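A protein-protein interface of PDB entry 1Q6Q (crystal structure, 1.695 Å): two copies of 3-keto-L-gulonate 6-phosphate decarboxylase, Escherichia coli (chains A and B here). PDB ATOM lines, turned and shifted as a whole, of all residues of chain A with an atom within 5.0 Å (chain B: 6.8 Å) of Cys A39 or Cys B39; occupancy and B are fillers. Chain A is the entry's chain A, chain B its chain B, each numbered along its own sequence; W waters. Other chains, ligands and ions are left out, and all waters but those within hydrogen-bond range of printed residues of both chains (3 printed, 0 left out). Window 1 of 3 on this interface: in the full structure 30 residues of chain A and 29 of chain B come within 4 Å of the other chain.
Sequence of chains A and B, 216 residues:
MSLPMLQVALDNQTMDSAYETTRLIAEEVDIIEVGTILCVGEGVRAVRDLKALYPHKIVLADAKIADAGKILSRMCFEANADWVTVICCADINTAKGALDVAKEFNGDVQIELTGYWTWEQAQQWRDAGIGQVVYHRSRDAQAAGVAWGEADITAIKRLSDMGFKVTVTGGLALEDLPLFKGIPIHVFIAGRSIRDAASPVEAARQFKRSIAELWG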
ATOM      1  N   VAL A  34       4.235  19.104   7.085  1.00  0.00           N
ATOM      2  CA  VAL A  34       3.711  17.855   7.554  1.00  0.00           C
ATOM      3  C   VAL A  34       3.332  18.120   9.008  1.00  0.00           C
ATOM      4  O   VAL A  34       4.174  18.223   9.869  1.00  0.00           O
ATOM      5  CB  VAL A  34       4.811  16.752   7.473  1.00  0.00           C
ATOM      6  CG1 VAL A  34       4.192  15.369   7.846  1.00  0.00           C
ATOM      7  CG2 VAL A  34       5.381  16.732   6.043  1.00  0.00           C
ATOM      8  N   GLY A  35       2.057  18.326   9.274  1.00  0.00           N
ATOM      9  CA  GLY A  35       1.608  18.673  10.593  1.00  0.00           C
ATOM     10  C   GLY A  35       1.847  17.556  11.561  1.00  0.00           C
ATOM     11  O   GLY A  35       1.980  16.389  11.197  1.00  0.00           O
ATOM     12  N   THR A  36       1.779  17.917  12.824  1.00  0.00           N
ATOM     13  CA  THR A  36       1.981  16.943  13.894  1.00  0.00           C
ATOM     14  C   THR A  36       0.974  15.798  13.766  1.00  0.00           C
ATOM     15  O   THR A  36       1.347  14.638  13.901  1.00  0.00           O
ATOM     16  CB  THR A  36       1.872  17.596  15.223  1.00  0.00           C
ATOM     17  OG1 THR A  36       2.590  18.857  15.200  1.00  0.00           O
ATOM     18  CG2 THR A  36       2.546  16.683  16.289  1.00  0.00           C
ATOM     19  N   ILE A  37      -0.267  16.135  13.400  1.00  0.00           N
ATOM     20  CA  ILE A  37      -1.332  15.152  13.244  1.00  0.00           C
ATOM     21  C   ILE A  37      -0.976  14.167  12.127  1.00  0.00           C
ATOM     22  O   ILE A  37      -1.246  12.983  12.229  1.00  0.00           O
ATOM     23  CB  ILE A  37      -2.674  15.913  12.962  1.00  0.00           C
ATOM     24  CG1 ILE A  37      -3.175  16.492  14.295  1.00  0.00           C
ATOM     25  CG2 ILE A  37      -3.729  15.032  12.393  1.00  0.00           C
ATOM     26  CD1 ILE A  37      -4.065  17.751  14.211  1.00  0.00           C
ATOM     27  N   LEU A  38      -0.358  14.660  11.052  1.00  0.00           N
ATOM     28  CA  LEU A  38       0.053  13.802   9.938  1.00  0.00           C
ATOM     29  C   LEU A  38       1.241  12.949  10.317  1.00  0.00           C
ATOM     30  O   LEU A  38       1.284  11.807   9.961  1.00  0.00           O
ATOM     31  CB  LEU A  38       0.262  14.611   8.660  1.00  0.00           C
ATOM     32  CG  LEU A  38       0.531  13.853   7.386  1.00  0.00           C
ATOM     33  CD1 LEU A  38      -0.593  12.849   7.098  1.00  0.00           C
ATOM     34  CD2 LEU A  38       0.687  14.807   6.236  1.00  0.00           C
ATOM     35  N   CYS A  39       2.183  13.515  11.044  1.00  0.00           N
ATOM     36  CA  CYS A  39       3.352  12.780  11.582  1.00  0.00           C
ATOM     37  C   CYS A  39       2.889  11.592  12.437  1.00  0.00           C
ATOM     38  O   CYS A  39       3.376  10.476  12.308  1.00  0.00           O
ATOM     39  CB  CYS A  39       4.207  13.696  12.441  1.00  0.00           C
ATOM     40  SG  CYS A  39       5.198  14.904  11.499  1.00  0.00           S
ATOM     41  N   VAL A  40       1.905  11.838  13.271  1.00  0.00           N
ATOM     42  CA  VAL A  40       1.394  10.805  14.139  1.00  0.00           C
ATOM     43  C   VAL A  40       0.501   9.824  13.381  1.00  0.00           C
ATOM     44  O   VAL A  40       0.481   8.638  13.714  1.00  0.00           O
ATOM     45  CB  VAL A  40       0.692  11.413  15.332  1.00  0.00           C
ATOM     46  CG1 VAL A  40      -0.111  10.372  16.090  1.00  0.00           C
ATOM     47  CG2 VAL A  40       1.711  12.052  16.236  1.00  0.00           C
ATOM     48  N   GLY A  41      -0.208  10.305  12.368  1.00  0.00           N
ATOM     49  CA  GLY A  41      -1.118   9.488  11.605  1.00  0.00           C
ATOM     50  C   GLY A  41      -0.395   8.496  10.746  1.00  0.00           C
ATOM     51  O   GLY A  41      -0.781   7.326  10.650  1.00  0.00           O
ATOM     52  N   GLU A  42       0.596   9.016  10.014  1.00  0.00           N
ATOM     53  CA  GLU A  42       1.274   8.231   8.980  1.00  0.00           C
ATOM     54  C   GLU A  42       2.729   7.911   9.282  1.00  0.00           C
ATOM     55  O   GLU A  42       3.302   7.018   8.604  1.00  0.00           O
ATOM     56  CB  GLU A  42       1.166   8.952   7.623  1.00  0.00           C
ATOM     57  CG  GLU A  42      -0.244   9.120   7.003  1.00  0.00           C
ATOM     58  CD  GLU A  42      -0.734   7.826   6.316  1.00  0.00           C
ATOM     59  OE1 GLU A  42      -0.164   6.731   6.586  1.00  0.00           O
ATOM     60  OE2 GLU A  42      -1.680   7.888   5.521  1.00  0.00           O
ATOM     61  N   GLY A  43       3.368   8.667  10.188  1.00  0.00           N
ATOM     62  CA  GLY A  43       4.800   8.568  10.426  1.00  0.00           C
ATOM     63  C   GLY A  43       5.612   9.248   9.353  1.00  0.00           C
ATOM     64  O   GLY A  43       5.031   9.983   8.505  1.00  0.00           O
ATOM     65  N   VAL A  44       6.926   9.106   9.419  1.00  0.00           N
ATOM     66  CA  VAL A  44       7.824   9.889   8.564  1.00  0.00           C
ATOM     67  C   VAL A  44       7.687   9.628   7.081  1.00  0.00           C
ATOM     68  O   VAL A  44       8.213  10.417   6.280  1.00  0.00           O
ATOM     69  CB  VAL A  44       9.322   9.738   8.937  1.00  0.00           C
ATOM     70  CG1 VAL A  44       9.652  10.563  10.138  1.00  0.00           C
ATOM     71  CG2 VAL A  44       9.692   8.302   9.102  1.00  0.00           C
ATOM     72  N   ALA A  61       8.775  19.353   8.857  1.00  0.00           N
ATOM     73  CA  ALA A  61       8.191  18.265   9.638  1.00  0.00           C
ATOM     74  C   ALA A  61       7.877  18.845  11.016  1.00  0.00           C
ATOM     75  O   ALA A  61       8.822  19.103  11.822  1.00  0.00           O
ATOM     76  CB  ALA A  61       9.185  17.111   9.769  1.00  0.00           C
ATOM     77  N   ASP A  62       6.589  19.050  11.302  1.00  0.00           N
ATOM     78  CA  ASP A  62       6.147  19.624  12.582  1.00  0.00           C
ATOM     79  C   ASP A  62       6.043  18.512  13.647  1.00  0.00           C
ATOM     80  O   ASP A  62       4.984  18.238  14.196  1.00  0.00           O
ATOM     81  CB  ASP A  62       4.816  20.426  12.425  1.00  0.00           C
ATOM     82  CG  ASP A  62       4.529  21.328  13.648  1.00  0.00           C
ATOM     83  OD1 ASP A  62       5.379  21.420  14.593  1.00  0.00           O
ATOM     84  OD2 ASP A  62       3.460  21.887  13.853  1.00  0.00           O
ATOM     85  N   ALA A  63       7.193  17.908  13.969  1.00  0.00           N
ATOM     86  CA  ALA A  63       7.286  16.766  14.872  1.00  0.00           C
ATOM     87  C   ALA A  63       7.219  17.141  16.329  1.00  0.00           C
ATOM     88  O   ALA A  63       6.923  16.305  17.196  1.00  0.00           O
ATOM     89  CB  ALA A  63       8.593  15.959  14.574  1.00  0.00           C
ATOM     90  N   LEU B  10       8.991   0.910  23.648  1.00  0.00           N
ATOM     91  CA  LEU B  10       9.361   0.551  22.285  1.00  0.00           C
ATOM     92  C   LEU B  10       9.682   1.821  21.484  1.00  0.00           C
ATOM     93  O   LEU B  10       8.879   2.343  20.708  1.00  0.00           O
ATOM     94  CB  LEU B  10       8.266  -0.292  21.640  1.00  0.00           C
ATOM     95  CG  LEU B  10       7.929  -1.550  22.413  1.00  0.00           C
ATOM     96  CD1 LEU B  10       6.669  -2.164  21.817  1.00  0.00           C
ATOM     97  CD2 LEU B  10       9.066  -2.605  22.392  1.00  0.00           C
ATOM     98  N   ASN B  12      11.478   2.257  18.886  1.00  0.00           N
ATOM     99  CA  ASN B  12      12.030   1.592  17.730  1.00  0.00           C
ATOM    100  C   ASN B  12      11.540   2.365  16.547  1.00  0.00           C
ATOM    101  O   ASN B  12      10.471   2.972  16.593  1.00  0.00           O
ATOM    102  CB  ASN B  12      11.489   0.146  17.671  1.00  0.00           C
ATOM    103  CG  ASN B  12      11.920  -0.694  18.777  1.00  0.00           C
ATOM    104  OD1 ASN B  12      12.846  -1.500  18.669  1.00  0.00           O
ATOM    105  ND2 ASN B  12      11.203  -0.604  19.853  1.00  0.00           N
ATOM    106  N   VAL B  34       4.164   2.132  23.060  1.00  0.00           N
ATOM    107  CA  VAL B  34       4.478   2.598  21.758  1.00  0.00           C
ATOM    108  C   VAL B  34       5.248   3.861  21.929  1.00  0.00           C
ATOM    109  O   VAL B  34       4.717   4.914  22.244  1.00  0.00           O
ATOM    110  CB  VAL B  34       3.213   2.815  20.913  1.00  0.00           C
ATOM    111  CG1 VAL B  34       3.638   3.129  19.477  1.00  0.00           C
ATOM    112  CG2 VAL B  34       2.358   1.586  20.944  1.00  0.00           C
ATOM    113  N   GLY B  35       6.557   3.765  21.803  1.00  0.00           N
ATOM    114  CA  GLY B  35       7.353   4.960  22.051  1.00  0.00           C
ATOM    115  C   GLY B  35       7.112   6.067  21.025  1.00  0.00           C
ATOM    116  O   GLY B  35       6.702   5.856  19.904  1.00  0.00           O
ATOM    117  N   THR B  36       7.423   7.282  21.452  1.00  0.00           N
ATOM    118  CA  THR B  36       7.370   8.413  20.600  1.00  0.00           C
ATOM    119  C   THR B  36       8.076   8.183  19.253  1.00  0.00           C
ATOM    120  O   THR B  36       7.566   8.597  18.195  1.00  0.00           O
ATOM    121  CB  THR B  36       7.949   9.624  21.322  1.00  0.00           C
ATOM    122  OG1 THR B  36       7.501   9.693  22.684  1.00  0.00           O
ATOM    123  CG2 THR B  36       7.541  10.922  20.642  1.00  0.00           C
ATOM    124  N   ILE B  37       9.244   7.508  19.294  1.00  0.00           N
ATOM    125  CA  ILE B  37      10.053   7.244  18.109  1.00  0.00           C
ATOM    126  C   ILE B  37       9.343   6.268  17.189  1.00  0.00           C
ATOM    127  O   ILE B  37       9.381   6.445  15.960  1.00  0.00           O
ATOM    128  CB  ILE B  37      11.494   6.702  18.537  1.00  0.00           C
ATOM    129  CG1 ILE B  37      12.312   7.909  19.071  1.00  0.00           C
ATOM    130  CG2 ILE B  37      12.161   5.991  17.438  1.00  0.00           C
ATOM    131  CD1 ILE B  37      13.437   7.576  20.153  1.00  0.00           C
ATOM    132  N   LEU B  38       8.593   5.337  17.758  1.00  0.00           N
ATOM    133  CA  LEU B  38       7.809   4.418  16.947  1.00  0.00           C
ATOM    134  C   LEU B  38       6.579   5.122  16.369  1.00  0.00           C
ATOM    135  O   LEU B  38       6.193   4.806  15.271  1.00  0.00           O
ATOM    136  CB  LEU B  38       7.433   3.193  17.689  1.00  0.00           C
ATOM    137  CG  LEU B  38       6.700   2.050  16.967  1.00  0.00           C
ATOM    138  CD1 LEU B  38       7.491   1.520  15.760  1.00  0.00           C
ATOM    139  CD2 LEU B  38       6.529   0.932  17.987  1.00  0.00           C
ATOM    140  N   CYS B  39       5.954   6.001  17.118  1.00  0.00           N
ATOM    141  CA  CYS B  39       4.783   6.773  16.646  1.00  0.00           C
ATOM    142  C   CYS B  39       5.221   7.587  15.448  1.00  0.00           C
ATOM    143  O   CYS B  39       4.520   7.627  14.440  1.00  0.00           O
ATOM    144  CB  CYS B  39       4.251   7.689  17.709  1.00  0.00           C
ATOM    145  SG  CYS B  39       3.437   6.937  19.168  1.00  0.00           S
ATOM    146  N   VAL B  40       6.391   8.212  15.534  1.00  0.00           N
ATOM    147  CA  VAL B  40       6.863   9.028  14.421  1.00  0.00           C
ATOM    148  C   VAL B  40       7.357   8.191  13.267  1.00  0.00           C
ATOM    149  O   VAL B  40       7.277   8.609  12.118  1.00  0.00           O
ATOM    150  CB  VAL B  40       7.944  10.033  14.938  1.00  0.00           C
ATOM    151  CG1 VAL B  40       8.673  10.717  13.765  1.00  0.00           C
ATOM    152  CG2 VAL B  40       7.284  11.034  15.833  1.00  0.00           C
ATOM    153  N   GLY B  41       7.894   7.017  13.530  1.00  0.00           N
ATOM    154  CA  GLY B  41       8.408   6.155  12.468  1.00  0.00           C
ATOM    155  C   GLY B  41       7.276   5.534  11.657  1.00  0.00           C
ATOM    156  O   GLY B  41       7.304   5.539  10.416  1.00  0.00           O
ATOM    157  N   GLU B  42       6.268   5.033  12.371  1.00  0.00           N
ATOM    158  CA  GLU B  42       5.233   4.216  11.724  1.00  0.00           C
ATOM    159  C   GLU B  42       3.842   4.806  11.757  1.00  0.00           C
ATOM    160  O   GLU B  42       2.953   4.336  11.041  1.00  0.00           O
ATOM    161  CB  GLU B  42       5.197   2.823  12.340  1.00  0.00           C
ATOM    162  CG  GLU B  42       6.416   1.952  12.156  1.00  0.00           C
ATOM    163  CD  GLU B  42       6.437   1.234  10.829  1.00  0.00           C
ATOM    164  OE1 GLU B  42       5.739   1.695   9.921  1.00  0.00           O
ATOM    165  OE2 GLU B  42       7.148   0.249  10.700  1.00  0.00           O
ATOM    166  N   GLY B  43       3.635   5.825  12.564  1.00  0.00           N
ATOM    167  CA  GLY B  43       2.315   6.337  12.814  1.00  0.00           C
ATOM    168  C   GLY B  43       1.482   5.460  13.723  1.00  0.00           C
ATOM    169  O   GLY B  43       1.943   4.462  14.285  1.00  0.00           O
ATOM    170  N   VAL B  44       0.209   5.800  13.811  1.00  0.00           N
ATOM    171  CA  VAL B  44      -0.664   5.265  14.815  1.00  0.00           C
ATOM    172  C   VAL B  44      -1.077   3.816  14.530  1.00  0.00           C
ATOM    173  O   VAL B  44      -1.589   3.121  15.409  1.00  0.00           O
ATOM    174  CB  VAL B  44      -1.814   6.268  14.983  1.00  0.00           C
ATOM    175  CG1 VAL B  44      -2.885   6.063  13.911  1.00  0.00           C
ATOM    176  CG2 VAL B  44      -2.279   6.260  16.356  1.00  0.00           C
ATOM    177  N   ALA B  46       0.991   1.697  14.657  1.00  0.00           N
ATOM    178  CA  ALA B  46       1.822   0.967  15.656  1.00  0.00           C
ATOM    179  C   ALA B  46       0.971   0.590  16.881  1.00  0.00           C
ATOM    180  O   ALA B  46       1.135  -0.470  17.467  1.00  0.00           O
ATOM    181  CB  ALA B  46       2.993   1.779  16.080  1.00  0.00           C
ATOM    182  N   VAL B  47       0.140   1.529  17.316  1.00  0.00           N
ATOM    183  CA  VAL B  47      -0.780   1.322  18.421  1.00  0.00           C
ATOM    184  C   VAL B  47      -1.803   0.204  18.109  1.00  0.00           C
ATOM    185  O   VAL B  47      -1.997  -0.750  18.912  1.00  0.00           O
ATOM    186  CB  VAL B  47      -1.479   2.666  18.786  1.00  0.00           C
ATOM    187  CG1 VAL B  47      -2.484   2.403  19.885  1.00  0.00           C
ATOM    188  CG2 VAL B  47      -0.474   3.726  19.202  1.00  0.00           C
ATOM    189  N   LEU B  60       0.259   1.799  25.940  1.00  0.00           N
ATOM    190  CA  LEU B  60       0.462   3.228  26.198  1.00  0.00           C
ATOM    191  C   LEU B  60       1.047   3.896  24.930  1.00  0.00           C
ATOM    192  O   LEU B  60       2.027   3.410  24.355  1.00  0.00           O
ATOM    193  CB  LEU B  60       1.443   3.424  27.316  1.00  0.00           C
ATOM    194  CG  LEU B  60       1.963   4.827  27.769  1.00  0.00           C
ATOM    195  CD1 LEU B  60       3.139   5.284  27.023  1.00  0.00           C
ATOM    196  CD2 LEU B  60       0.901   5.892  27.726  1.00  0.00           C
ATOM    197  N   ALA B  61       0.369   4.904  24.379  1.00  0.00           N
ATOM    198  CA  ALA B  61       0.950   5.637  23.262  1.00  0.00           C
ATOM    199  C   ALA B  61       1.687   6.862  23.744  1.00  0.00           C
ATOM    200  O   ALA B  61       1.083   7.804  24.257  1.00  0.00           O
ATOM    201  CB  ALA B  61      -0.153   6.030  22.226  1.00  0.00           C
ATOM    202  N   ASP B  62       2.994   6.849  23.663  1.00  0.00           N
ATOM    203  CA  ASP B  62       3.799   7.979  24.127  1.00  0.00           C
ATOM    204  C   ASP B  62       3.909   9.084  23.076  1.00  0.00           C
ATOM    205  O   ASP B  62       4.974   9.458  22.548  1.00  0.00           O
ATOM    206  CB  ASP B  62       5.168   7.478  24.659  1.00  0.00           C
ATOM    207  CG  ASP B  62       5.909   8.561  25.421  1.00  0.00           C
ATOM    208  OD1 ASP B  62       5.327   9.659  25.691  1.00  0.00           O
ATOM    209  OD2 ASP B  62       7.102   8.460  25.743  1.00  0.00           O
ATOM    210  N   ALA B  63       2.744   9.675  22.783  1.00  0.00           N
ATOM    211  CA  ALA B  63       2.609  10.657  21.740  1.00  0.00           C
ATOM    212  C   ALA B  63       3.086  12.049  22.125  1.00  0.00           C
ATOM    213  O   ALA B  63       3.362  12.877  21.253  1.00  0.00           O
ATOM    214  CB  ALA B  63       1.153  10.736  21.302  1.00  0.00           C
ATOM    215  N   CYS B  76      -5.232   8.289  18.686  1.00  0.00           N
ATOM    216  CA  CYS B  76      -4.658   7.208  19.512  1.00  0.00           C
ATOM    217  C   CYS B  76      -5.665   6.257  20.096  1.00  0.00           C
ATOM    218  O   CYS B  76      -5.493   5.029  20.082  1.00  0.00           O
ATOM    219  CB  CYS B  76      -3.806   7.777  20.631  1.00  0.00           C
ATOM    220  SG  CYS B  76      -2.380   8.699  20.030  1.00  0.00           S
HETATM  221  O   HOH W   1       6.031   6.062   8.220  1.00  0.00           O
HETATM  222  O   HOH W   2      -0.019   4.685  10.775  1.00  0.00           O
HETATM  223  O   HOH W   3       5.416  13.749  18.677  1.00  0.00           O
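The backbone NH of Val A44 is in hydrogen-bond range of the backbone carbonyl oxygen of Val B40, 2.8 Å away. The backbone carbonyl oxygen (O) of Val A40 is in hydrogen-bond range of the backbone NH (N) of Val B44 (2.9 Å).
The backbone carbonyl oxygen (O) of Gly B35 lies within hydrogen-bond range of the side-chain sulfur (SG) of Cys B39 (3.5 Å). SG of Cys A39 lies within hydrogen-bond range of O of Gly A35 (3.6 Å).
Cys A39 touches Cys B39 (O to O, 3.7 Å). CA of Gly B43 touches O of Val A40, at 3.1 Å. Gly A41 touches Gly B43. Gly A41 touches Val B44 (O to N, 3.6 Å). Glu B42 touches Glu A42. Gly B43 touches Glu A42 (CA to C, 3.9 Å). Gly A43 touches Val B40. Gly A43 touches Gly B41. N of Gly A43 touches CA of Gly B43, at 3.7 Å. Val A44 touches Gly B41.
Of the printed residues of chain B, Cys A39 touches Cys B39. Of the printed residues of chain B, Gly A43 touches Val B40, Gly B41 and Gly B43. Of the printed residues of chain A, Val B44 touches Val A40 (2.9 Å) and Gly A41 (3.6 Å). Of the printed residues of chain B, Glu A42 touches Glu B42 and Gly B43. Printed residues of chain B within 4 Å of Val A40: Gly B43 (3.1 Å) and Val B44 (2.9 Å). Of the printed residues of chain A, Gly B41 touches Gly A43 and Val A44. Thr A36 touches none of the printed residues of chain B. Leu B10 touches none of the printed residues of chain A. The nearest residue of chain A that does not touch Cys B39 is Gly A43 (4.1 Å).
Of the 20 printed residues of chain B, 6 touch a printed residue of chain A. Hydrophobic or aromatic side chains of chain B within 4 Å of the printed part of chain A: Val B40 and Val B44. Among the printed residues, 12 pairs touch across the chains.
Cys A39 touches its own counterpart, Cys B39. Val A40 touches Val B44, and with the chains exchanged Val A44 touches Val B40. Gly A41 touches Gly B43, and with the chains exchanged Gly A43 touches Gly B41. Glu A42 touches Gly B43, but with the chains exchanged Gly A43 does not touch Glu B42 (4.1 Å).
Water W1 lies within hydrogen-bond range of O of Gly B41 (2.6 Å), O of Glu A42 (2.9 Å) and N of Val A44 (3.4 Å). Water W2 lies within hydrogen-bond range of the backbone carbonyl oxygen (O) of Gly A41 (2.8 Å), the backbone carbonyl oxygen (O) of Glu B42 (3.0 Å) and the backbone NH (N) of Val B44 (3.2 Å). Water W3 bridges the backbone carbonyl oxygen (O) of Ala A63 (3.3 Å) and the backbone carbonyl oxygen (O) of Ala B63 (3.4 Å).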
